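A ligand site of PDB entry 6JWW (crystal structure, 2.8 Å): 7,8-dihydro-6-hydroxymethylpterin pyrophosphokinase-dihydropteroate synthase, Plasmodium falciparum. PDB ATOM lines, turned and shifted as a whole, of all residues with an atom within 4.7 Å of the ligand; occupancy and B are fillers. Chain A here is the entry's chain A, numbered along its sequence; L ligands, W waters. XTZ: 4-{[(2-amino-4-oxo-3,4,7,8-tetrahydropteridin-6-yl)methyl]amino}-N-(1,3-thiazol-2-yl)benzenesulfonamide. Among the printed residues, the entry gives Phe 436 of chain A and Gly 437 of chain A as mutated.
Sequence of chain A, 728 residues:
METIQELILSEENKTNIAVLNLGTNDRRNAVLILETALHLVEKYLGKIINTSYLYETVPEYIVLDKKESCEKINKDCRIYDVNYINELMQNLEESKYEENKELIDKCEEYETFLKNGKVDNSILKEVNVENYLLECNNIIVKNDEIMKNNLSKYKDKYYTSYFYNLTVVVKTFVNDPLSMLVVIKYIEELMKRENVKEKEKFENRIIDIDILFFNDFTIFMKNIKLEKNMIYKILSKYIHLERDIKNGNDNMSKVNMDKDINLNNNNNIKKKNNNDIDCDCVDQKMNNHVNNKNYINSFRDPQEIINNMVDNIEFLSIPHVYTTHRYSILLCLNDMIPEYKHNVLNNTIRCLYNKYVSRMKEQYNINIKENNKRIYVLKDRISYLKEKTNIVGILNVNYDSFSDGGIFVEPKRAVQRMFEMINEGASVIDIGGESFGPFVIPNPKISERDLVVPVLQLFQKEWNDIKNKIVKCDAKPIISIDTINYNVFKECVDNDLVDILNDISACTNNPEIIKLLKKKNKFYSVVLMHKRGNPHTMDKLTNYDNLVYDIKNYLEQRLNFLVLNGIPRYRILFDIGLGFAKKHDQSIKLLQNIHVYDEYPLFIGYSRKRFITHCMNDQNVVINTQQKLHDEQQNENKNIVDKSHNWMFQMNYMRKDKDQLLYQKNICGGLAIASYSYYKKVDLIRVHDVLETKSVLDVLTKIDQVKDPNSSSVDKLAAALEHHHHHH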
ATOM      1  N   PHE A 436      12.554  27.187 -24.887  1.00  0.00           N
ATOM      2  CA  PHE A 436      11.902  25.884 -24.689  1.00  0.00           C
ATOM      3  C   PHE A 436      10.898  25.786 -23.526  1.00  0.00           C
ATOM      4  O   PHE A 436       9.793  25.257 -23.701  1.00  0.00           O
ATOM      5  CB  PHE A 436      12.953  24.769 -24.541  1.00  0.00           C
ATOM      6  CG  PHE A 436      14.070  24.841 -25.553  1.00  0.00           C
ATOM      7  CD1 PHE A 436      13.887  24.322 -26.850  1.00  0.00           C
ATOM      8  CD2 PHE A 436      15.285  25.444 -25.226  1.00  0.00           C
ATOM      9  CE1 PHE A 436      14.918  24.390 -27.778  1.00  0.00           C
ATOM     10  CE2 PHE A 436      16.307  25.527 -26.168  1.00  0.00           C
ATOM     11  CZ  PHE A 436      16.122  24.986 -27.444  1.00  0.00           C
ATOM     12  N   GLY A 437      11.293  26.278 -22.351  1.00  0.00           N
ATOM     13  CA  GLY A 437      10.474  26.231 -21.136  1.00  0.00           C
ATOM     14  C   GLY A 437      10.609  24.917 -20.395  1.00  0.00           C
ATOM     15  O   GLY A 437       9.619  24.354 -19.935  1.00  0.00           O
ATOM     16  N   ASP A 482      16.680  22.342 -35.469  1.00  0.00           N
ATOM     17  CA  ASP A 482      15.504  22.371 -34.628  1.00  0.00           C
ATOM     18  C   ASP A 482      14.712  23.659 -34.864  1.00  0.00           C
ATOM     19  O   ASP A 482      14.841  24.628 -34.125  1.00  0.00           O
ATOM     20  CB  ASP A 482      15.937  22.253 -33.163  1.00  0.00           C
ATOM     21  CG  ASP A 482      14.782  22.088 -32.200  1.00  0.00           C
ATOM     22  OD1 ASP A 482      13.618  22.392 -32.550  1.00  0.00           O
ATOM     23  OD2 ASP A 482      15.029  21.621 -31.063  1.00  0.00           O
ATOM     24  N   ASN A 502      14.196  19.078 -37.674  1.00  0.00           N
ATOM     25  CA  ASN A 502      13.639  18.697 -36.386  1.00  0.00           C
ATOM     26  C   ASN A 502      12.452  19.618 -36.065  1.00  0.00           C
ATOM     27  O   ASN A 502      12.614  20.653 -35.409  1.00  0.00           O
ATOM     28  CB  ASN A 502      14.726  18.727 -35.307  1.00  0.00           C
ATOM     29  CG  ASN A 502      14.227  18.314 -33.922  1.00  0.00           C
ATOM     30  OD1 ASN A 502      13.065  17.946 -33.729  1.00  0.00           O
ATOM     31  ND2 ASN A 502      15.124  18.388 -32.948  1.00  0.00           N
ATOM     32  N   ILE A 504       9.229  20.421 -34.082  1.00  0.00           N
ATOM     33  CA  ILE A 504       8.603  20.048 -32.811  1.00  0.00           C
ATOM     34  C   ILE A 504       7.074  20.144 -32.814  1.00  0.00           C
ATOM     35  O   ILE A 504       6.412  19.763 -31.846  1.00  0.00           O
ATOM     36  CB  ILE A 504       9.191  20.840 -31.597  1.00  0.00           C
ATOM     37  CG1 ILE A 504       8.851  22.342 -31.694  1.00  0.00           C
ATOM     38  CG2 ILE A 504      10.683  20.581 -31.429  1.00  0.00           C
ATOM     39  CD1 ILE A 504       8.788  23.044 -30.360  1.00  0.00           C
ATOM     40  N   VAL A 527      12.359  14.793 -38.168  1.00  0.00           N
ATOM     41  CA  VAL A 527      11.874  14.285 -36.887  1.00  0.00           C
ATOM     42  C   VAL A 527      10.492  14.897 -36.682  1.00  0.00           C
ATOM     43  O   VAL A 527      10.306  16.092 -36.877  1.00  0.00           O
ATOM     44  CB  VAL A 527      12.828  14.635 -35.724  1.00  0.00           C
ATOM     45  CG1 VAL A 527      12.374  13.960 -34.435  1.00  0.00           C
ATOM     46  CG2 VAL A 527      14.252  14.212 -36.059  1.00  0.00           C
ATOM     47  N   MET A 529       7.810  15.468 -33.903  1.00  0.00           N
ATOM     48  CA  MET A 529       7.573  15.470 -32.482  1.00  0.00           C
ATOM     49  C   MET A 529       6.126  15.776 -32.180  1.00  0.00           C
ATOM     50  O   MET A 529       5.488  16.546 -32.905  1.00  0.00           O
ATOM     51  CB  MET A 529       8.488  16.484 -31.790  1.00  0.00           C
ATOM     52  CG  MET A 529       8.776  16.096 -30.345  1.00  0.00           C
ATOM     53  SD  MET A 529       9.211  17.441 -29.221  1.00  0.00           S
ATOM     54  CE  MET A 529       7.660  18.314 -29.096  1.00  0.00           C
ATOM     55  N   MET A 538       1.407  25.040 -22.510  1.00  0.00           N
ATOM     56  CA  MET A 538       1.810  23.633 -22.428  1.00  0.00           C
ATOM     57  C   MET A 538       1.371  22.763 -21.235  1.00  0.00           C
ATOM     58  O   MET A 538       0.844  21.678 -21.434  1.00  0.00           O
ATOM     59  CB  MET A 538       3.336  23.599 -22.521  1.00  0.00           C
ATOM     60  CG  MET A 538       3.898  22.329 -23.083  1.00  0.00           C
ATOM     61  SD  MET A 538       5.290  22.685 -24.153  1.00  0.00           S
ATOM     62  CE  MET A 538       6.648  22.663 -22.980  1.00  0.00           C
ATOM     63  N   ASP A 539       1.608  23.239 -20.015  1.00  0.00           N
ATOM     64  CA  ASP A 539       1.405  22.425 -18.803  1.00  0.00           C
ATOM     65  C   ASP A 539      -0.056  22.327 -18.388  1.00  0.00           C
ATOM     66  O   ASP A 539      -0.402  21.633 -17.422  1.00  0.00           O
ATOM     67  CB  ASP A 539       2.256  22.962 -17.654  1.00  0.00           C
ATOM     68  CG  ASP A 539       3.585  23.501 -18.111  1.00  0.00           C
ATOM     69  OD1 ASP A 539       3.586  24.526 -18.838  1.00  0.00           O
ATOM     70  OD2 ASP A 539       4.624  22.901 -17.741  1.00  0.00           O
ATOM     71  N   ASP A 575       8.908  10.946 -32.475  1.00  0.00           N
ATOM     72  CA  ASP A 575       9.318  11.530 -31.196  1.00  0.00           C
ATOM     73  C   ASP A 575       8.103  11.810 -30.321  1.00  0.00           C
ATOM     74  O   ASP A 575       7.203  12.568 -30.686  1.00  0.00           O
ATOM     75  CB  ASP A 575      10.152  12.792 -31.442  1.00  0.00           C
ATOM     76  CG  ASP A 575      10.801  13.348 -30.178  1.00  0.00           C
ATOM     77  OD1 ASP A 575      10.423  12.946 -29.046  1.00  0.00           O
ATOM     78  OD2 ASP A 575      11.691  14.207 -30.315  1.00  0.00           O
ATOM     79  N   LEU A 578       8.635  14.215 -24.882  1.00  0.00           N
ATOM     80  CA  LEU A 578       8.715  14.228 -23.412  1.00  0.00           C
ATOM     81  C   LEU A 578       8.733  15.644 -22.846  1.00  0.00           C
ATOM     82  O   LEU A 578       9.480  16.501 -23.340  1.00  0.00           O
ATOM     83  CB  LEU A 578       9.962  13.482 -22.933  1.00  0.00           C
ATOM     84  CG  LEU A 578      10.050  11.984 -23.245  1.00  0.00           C
ATOM     85  CD1 LEU A 578      11.486  11.530 -23.071  1.00  0.00           C
ATOM     86  CD2 LEU A 578       9.081  11.141 -22.408  1.00  0.00           C
ATOM     87  N   GLY A 579       7.909  15.873 -21.831  1.00  0.00           N
ATOM     88  CA  GLY A 579       7.736  17.196 -21.213  1.00  0.00           C
ATOM     89  C   GLY A 579       6.977  18.271 -21.988  1.00  0.00           C
ATOM     90  O   GLY A 579       6.874  19.405 -21.508  1.00  0.00           O
ATOM     91  N   PHE A 580       6.473  17.961 -23.180  1.00  0.00           N
ATOM     92  CA  PHE A 580       5.671  18.898 -23.964  1.00  0.00           C
ATOM     93  C   PHE A 580       4.199  18.550 -23.870  1.00  0.00           C
ATOM     94  O   PHE A 580       3.731  17.652 -24.578  1.00  0.00           O
ATOM     95  CB  PHE A 580       6.065  18.834 -25.433  1.00  0.00           C
ATOM     96  CG  PHE A 580       7.404  19.421 -25.746  1.00  0.00           C
ATOM     97  CD1 PHE A 580       8.565  18.642 -25.665  1.00  0.00           C
ATOM     98  CD2 PHE A 580       7.512  20.746 -26.188  1.00  0.00           C
ATOM     99  CE1 PHE A 580       9.802  19.174 -25.986  1.00  0.00           C
ATOM    100  CE2 PHE A 580       8.744  21.286 -26.511  1.00  0.00           C
ATOM    101  CZ  PHE A 580       9.891  20.500 -26.415  1.00  0.00           C
ATOM    102  N   HIS A 584       4.706  15.099 -15.325  1.00  0.00           N
ATOM    103  CA  HIS A 584       5.865  14.232 -15.087  1.00  0.00           C
ATOM    104  C   HIS A 584       5.589  12.735 -15.090  1.00  0.00           C
ATOM    105  O   HIS A 584       6.392  11.960 -15.600  1.00  0.00           O
ATOM    106  CB  HIS A 584       6.544  14.614 -13.793  1.00  0.00           C
ATOM    107  CG  HIS A 584       7.020  16.034 -13.778  1.00  0.00           C
ATOM    108  ND1 HIS A 584       7.369  16.704 -14.936  1.00  0.00           N
ATOM    109  CD2 HIS A 584       7.215  16.896 -12.770  1.00  0.00           C
ATOM    110  CE1 HIS A 584       7.754  17.917 -14.629  1.00  0.00           C
ATOM    111  NE2 HIS A 584       7.681  18.066 -13.312  1.00  0.00           N
ATOM    112  N   PHE A 603      13.153   8.619 -31.776  1.00  0.00           N
ATOM    113  CA  PHE A 603      14.002   9.727 -31.494  1.00  0.00           C
ATOM    114  C   PHE A 603      13.384  10.307 -30.240  1.00  0.00           C
ATOM    115  O   PHE A 603      12.191  10.600 -30.226  1.00  0.00           O
ATOM    116  CB  PHE A 603      13.871  10.711 -32.660  1.00  0.00           C
ATOM    117  CG  PHE A 603      14.774  11.911 -32.570  1.00  0.00           C
ATOM    118  CD1 PHE A 603      14.566  12.896 -31.586  1.00  0.00           C
ATOM    119  CD2 PHE A 603      15.811  12.091 -33.482  1.00  0.00           C
ATOM    120  CE1 PHE A 603      15.390  14.005 -31.518  1.00  0.00           C
ATOM    121  CE2 PHE A 603      16.639  13.200 -33.423  1.00  0.00           C
ATOM    122  CZ  PHE A 603      16.425  14.157 -32.432  1.00  0.00           C
ATOM    123  N   GLY A 605      13.999  12.937 -26.567  1.00  0.00           N
ATOM    124  CA  GLY A 605      14.746  13.944 -25.856  1.00  0.00           C
ATOM    125  C   GLY A 605      14.312  13.969 -24.414  1.00  0.00           C
ATOM    126  O   GLY A 605      13.233  14.455 -24.104  1.00  0.00           O
ATOM    127  N   LYS A 609      15.357  17.436 -18.590  1.00  0.00           N
ATOM    128  CA  LYS A 609      13.959  17.789 -18.439  1.00  0.00           C
ATOM    129  C   LYS A 609      13.526  17.651 -16.990  1.00  0.00           C
ATOM    130  O   LYS A 609      14.118  16.897 -16.219  1.00  0.00           O
ATOM    131  CB  LYS A 609      13.067  17.047 -19.427  1.00  0.00           C
ATOM    132  CG  LYS A 609      13.073  17.751 -20.772  1.00  0.00           C
ATOM    133  CD  LYS A 609      12.435  16.958 -21.898  1.00  0.00           C
ATOM    134  CE  LYS A 609      12.669  17.704 -23.207  1.00  0.00           C
ATOM    135  NZ  LYS A 609      12.308  16.941 -24.428  1.00  0.00           N
ATOM    136  N   ARG A 610      12.510  18.427 -16.638  1.00  0.00           N
ATOM    137  CA  ARG A 610      11.962  18.555 -15.303  1.00  0.00           C
ATOM    138  C   ARG A 610      11.559  17.224 -14.675  1.00  0.00           C
ATOM    139  O   ARG A 610      11.651  17.059 -13.463  1.00  0.00           O
ATOM    140  CB  ARG A 610      10.732  19.455 -15.407  1.00  0.00           C
ATOM    141  CG  ARG A 610      10.569  20.494 -14.308  1.00  0.00           C
ATOM    142  CD  ARG A 610      11.437  21.711 -14.575  1.00  0.00           C
ATOM    143  NE  ARG A 610      10.709  22.881 -15.089  1.00  0.00           N
ATOM    144  CZ  ARG A 610      11.154  24.136 -14.983  1.00  0.00           C
ATOM    145  NH1 ARG A 610      12.312  24.386 -14.375  1.00  0.00           N
ATOM    146  NH2 ARG A 610      10.448  25.147 -15.482  1.00  0.00           N
ATOM    147  N   PHE A 611      11.110  16.283 -15.506  1.00  0.00           N
ATOM    148  CA  PHE A 611      10.505  15.029 -15.020  1.00  0.00           C
ATOM    149  C   PHE A 611      11.530  14.049 -14.449  1.00  0.00           C
ATOM    150  O   PHE A 611      11.173  13.187 -13.643  1.00  0.00           O
ATOM    151  CB  PHE A 611       9.675  14.374 -16.142  1.00  0.00           C
ATOM    152  CG  PHE A 611      10.507  13.617 -17.134  1.00  0.00           C
ATOM    153  CD1 PHE A 611      11.070  14.257 -18.242  1.00  0.00           C
ATOM    154  CD2 PHE A 611      10.750  12.241 -16.964  1.00  0.00           C
ATOM    155  CE1 PHE A 611      11.841  13.551 -19.160  1.00  0.00           C
ATOM    156  CE2 PHE A 611      11.510  11.528 -17.876  1.00  0.00           C
ATOM    157  CZ  PHE A 611      12.065  12.190 -18.976  1.00  0.00           C
ATOM    158  N   ARG A 686      18.521  12.640 -27.914  1.00  0.00           N
ATOM    159  CA  ARG A 686      18.921  14.033 -28.026  1.00  0.00           C
ATOM    160  C   ARG A 686      19.479  14.507 -26.670  1.00  0.00           C
ATOM    161  O   ARG A 686      18.710  14.734 -25.719  1.00  0.00           O
ATOM    162  CB  ARG A 686      17.721  14.871 -28.442  1.00  0.00           C
ATOM    163  CG  ARG A 686      18.053  16.111 -29.250  1.00  0.00           C
ATOM    164  CD  ARG A 686      16.829  17.014 -29.406  1.00  0.00           C
ATOM    165  NE  ARG A 686      16.695  17.905 -28.267  1.00  0.00           N
ATOM    166  CZ  ARG A 686      16.879  19.229 -28.314  1.00  0.00           C
ATOM    167  NH1 ARG A 686      17.202  19.834 -29.441  1.00  0.00           N
ATOM    168  NH2 ARG A 686      16.756  19.936 -27.218  1.00  0.00           N
HETATM  169  O3  XTZ L   1      12.366  16.260 -26.847  1.00  0.00           O
HETATM  170  C16 XTZ L   1      12.631  16.929 -27.867  1.00  0.00           C
HETATM  171  N2  XTZ L   1      12.568  16.417 -29.095  1.00  0.00           N
HETATM  172  C3  XTZ L   1      13.046  18.334 -27.736  1.00  0.00           C
HETATM  173  N4  XTZ L   1      13.144  18.930 -26.535  1.00  0.00           N
HETATM  174  C4  XTZ L   1      13.500  20.230 -26.442  1.00  0.00           C
HETATM  175  C15 XTZ L   1      13.850  21.080 -27.648  1.00  0.00           C
HETATM  176  N8  XTZ L   1      13.743  20.368 -28.920  1.00  0.00           N
HETATM  177  C2  XTZ L   1      13.361  19.083 -28.981  1.00  0.00           C
HETATM  178  N3  XTZ L   1      13.254  18.436 -30.154  1.00  0.00           N
HETATM  179  C1  XTZ L   1      12.864  17.137 -30.197  1.00  0.00           C
HETATM  180  N1  XTZ L   1      12.782  16.540 -31.403  1.00  0.00           N
HETATM  181  C5  XTZ L   1      13.602  20.815 -25.057  1.00  0.00           C
HETATM  182  N5  XTZ L   1      12.402  21.480 -24.597  1.00  0.00           N
HETATM  183  C6  XTZ L   1      12.007  21.340 -23.305  1.00  0.00           C
HETATM  184  C14 XTZ L   1      12.887  21.618 -22.246  1.00  0.00           C
HETATM  185  C13 XTZ L   1      12.460  21.458 -20.935  1.00  0.00           C
HETATM  186  C9  XTZ L   1      11.170  21.021 -20.686  1.00  0.00           C
HETATM  187  C8  XTZ L   1      10.287  20.743 -21.735  1.00  0.00           C
HETATM  188  C7  XTZ L   1      10.706  20.896 -23.049  1.00  0.00           C
HETATM  189  S1  XTZ L   1      10.650  20.816 -19.187  1.00  0.00           S
HETATM  190  O1  XTZ L   1      11.464  21.540 -18.240  1.00  0.00           O
HETATM  191  O2  XTZ L   1      10.673  19.430 -18.866  1.00  0.00           O
HETATM  192  N6  XTZ L   1       9.109  21.288 -19.143  1.00  0.00           N
HETATM  193  C10 XTZ L   1       8.441  21.653 -18.021  1.00  0.00           C
HETATM  194  S2  XTZ L   1       8.629  23.174 -17.214  1.00  0.00           S
HETATM  195  C12 XTZ L   1       7.457  22.782 -15.995  1.00  0.00           C
HETATM  196  C11 XTZ L   1       6.995  21.498 -16.302  1.00  0.00           C
HETATM  197  N7  XTZ L   1       7.514  20.869 -17.413  1.00  0.00           N
HETATM  198  O   HOH W   1       4.727  19.755 -17.259  1.00  0.00           O
HETATM  199  O   HOH W   2      16.025  18.013 -25.068  1.00  0.00           O
HETATM  200  O   HOH W   3      15.672  21.731 -20.503  1.00  0.00           O
HETATM  201  O   HOH W   4       9.774  17.101 -18.155  1.00  0.00           O
HETATM  202  O   HOH W   5      11.129  13.767 -26.690  1.00  0.00           O
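NZ of Lys 609 lies within hydrogen-bond range of O of Gly 605 (2.7 Å). The side-chain amino group of Lys 609 lies within hydrogen-bond range of the backbone carbonyl oxygen of Leu 578, at 3.1 Å. The guanidinium group of Arg 686 is in salt-bridge range of the side-chain carboxylate of Asp 482.
The side-chain amino group (NZ) of Lys 609 lies within hydrogen-bond range of an oxygen (O3) of the ligand, 2.5 Å away. The side-chain carboxylate (OD2) of Asp 575 lies within hydrogen-bond range of a nitrogen (N2) of the ligand, at 2.7 Å. A nitrogen (N1) of the ligand sits at hydrogen-bond distance from the side-chain amide oxygen (OD1) of Asn 502 (2.7 Å). OD2 of Asp 482 sits at hydrogen-bond distance from N8 of the ligand. The backbone NH (N) of Arg 610 sits at hydrogen-bond distance from an oxygen (O2) of the ligand, 3.1 Å away. The guanidinium group of Arg 610 sits close to a sulfur (S2) of the ligand (3.0 Å). The backbone carbonyl oxygen (O) of Gly 437 sits at hydrogen-bond distance from a nitrogen (N6) of the ligand (3.2 Å). N8 of the ligand sits close to NH2 of Arg 686 (3.5 Å). The side-chain sulfur (SD) of Met 529 lies within hydrogen-bond range of a nitrogen (N2) of the ligand, 3.5 Å away.
O of Gly 605 sits close to O3 of the ligand (3.4 Å). Phe 436 touches the ligand (CB to N5, 3.3 Å). Ile 504 touches the ligand. OD2 of Asp 539 touches C11 of the ligand, at 3.1 Å. Gly 579 touches the ligand (O to C8, 3.7 Å). Phe 580 touches the ligand. Phe 603 touches the ligand (CE1 to N1, 3.6 Å). Hydrophobic or aromatic side chains within 4 Å of the ligand: Phe 436, Ile 504, Met 529, Phe 580 and Phe 603. Within 4 Å of the ligand: Phe 436, Gly 437, Asp 482, Asn 502, Ile 504, Met 529, Asp 539, Asp 575, Gly 579, Phe 580, Phe 603, Gly 605, Lys 609, Arg 610 and Arg 686.
Water W4 lies within hydrogen-bond range of an oxygen (O2) of the ligand (2.6 Å), the backbone NH (N) of Phe 611 (3.1 Å) and the backbone NH (N) of Arg 610 (3.4 Å). Water W5 lies within hydrogen-bond range of the side-chain carboxylate of Asp 575, an oxygen (O3) of the ligand, the backbone NH of Gly 605 and the backbone NH of Leu 578. Water W1 bridges a nitrogen (N7) of the ligand (3.0 Å) and the side-chain carboxylate of Asp 539 (3.2 Å). Water W2 bridges NH2 of Arg 686 (3.0 Å) and N4 of the ligand (3.4 Å).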
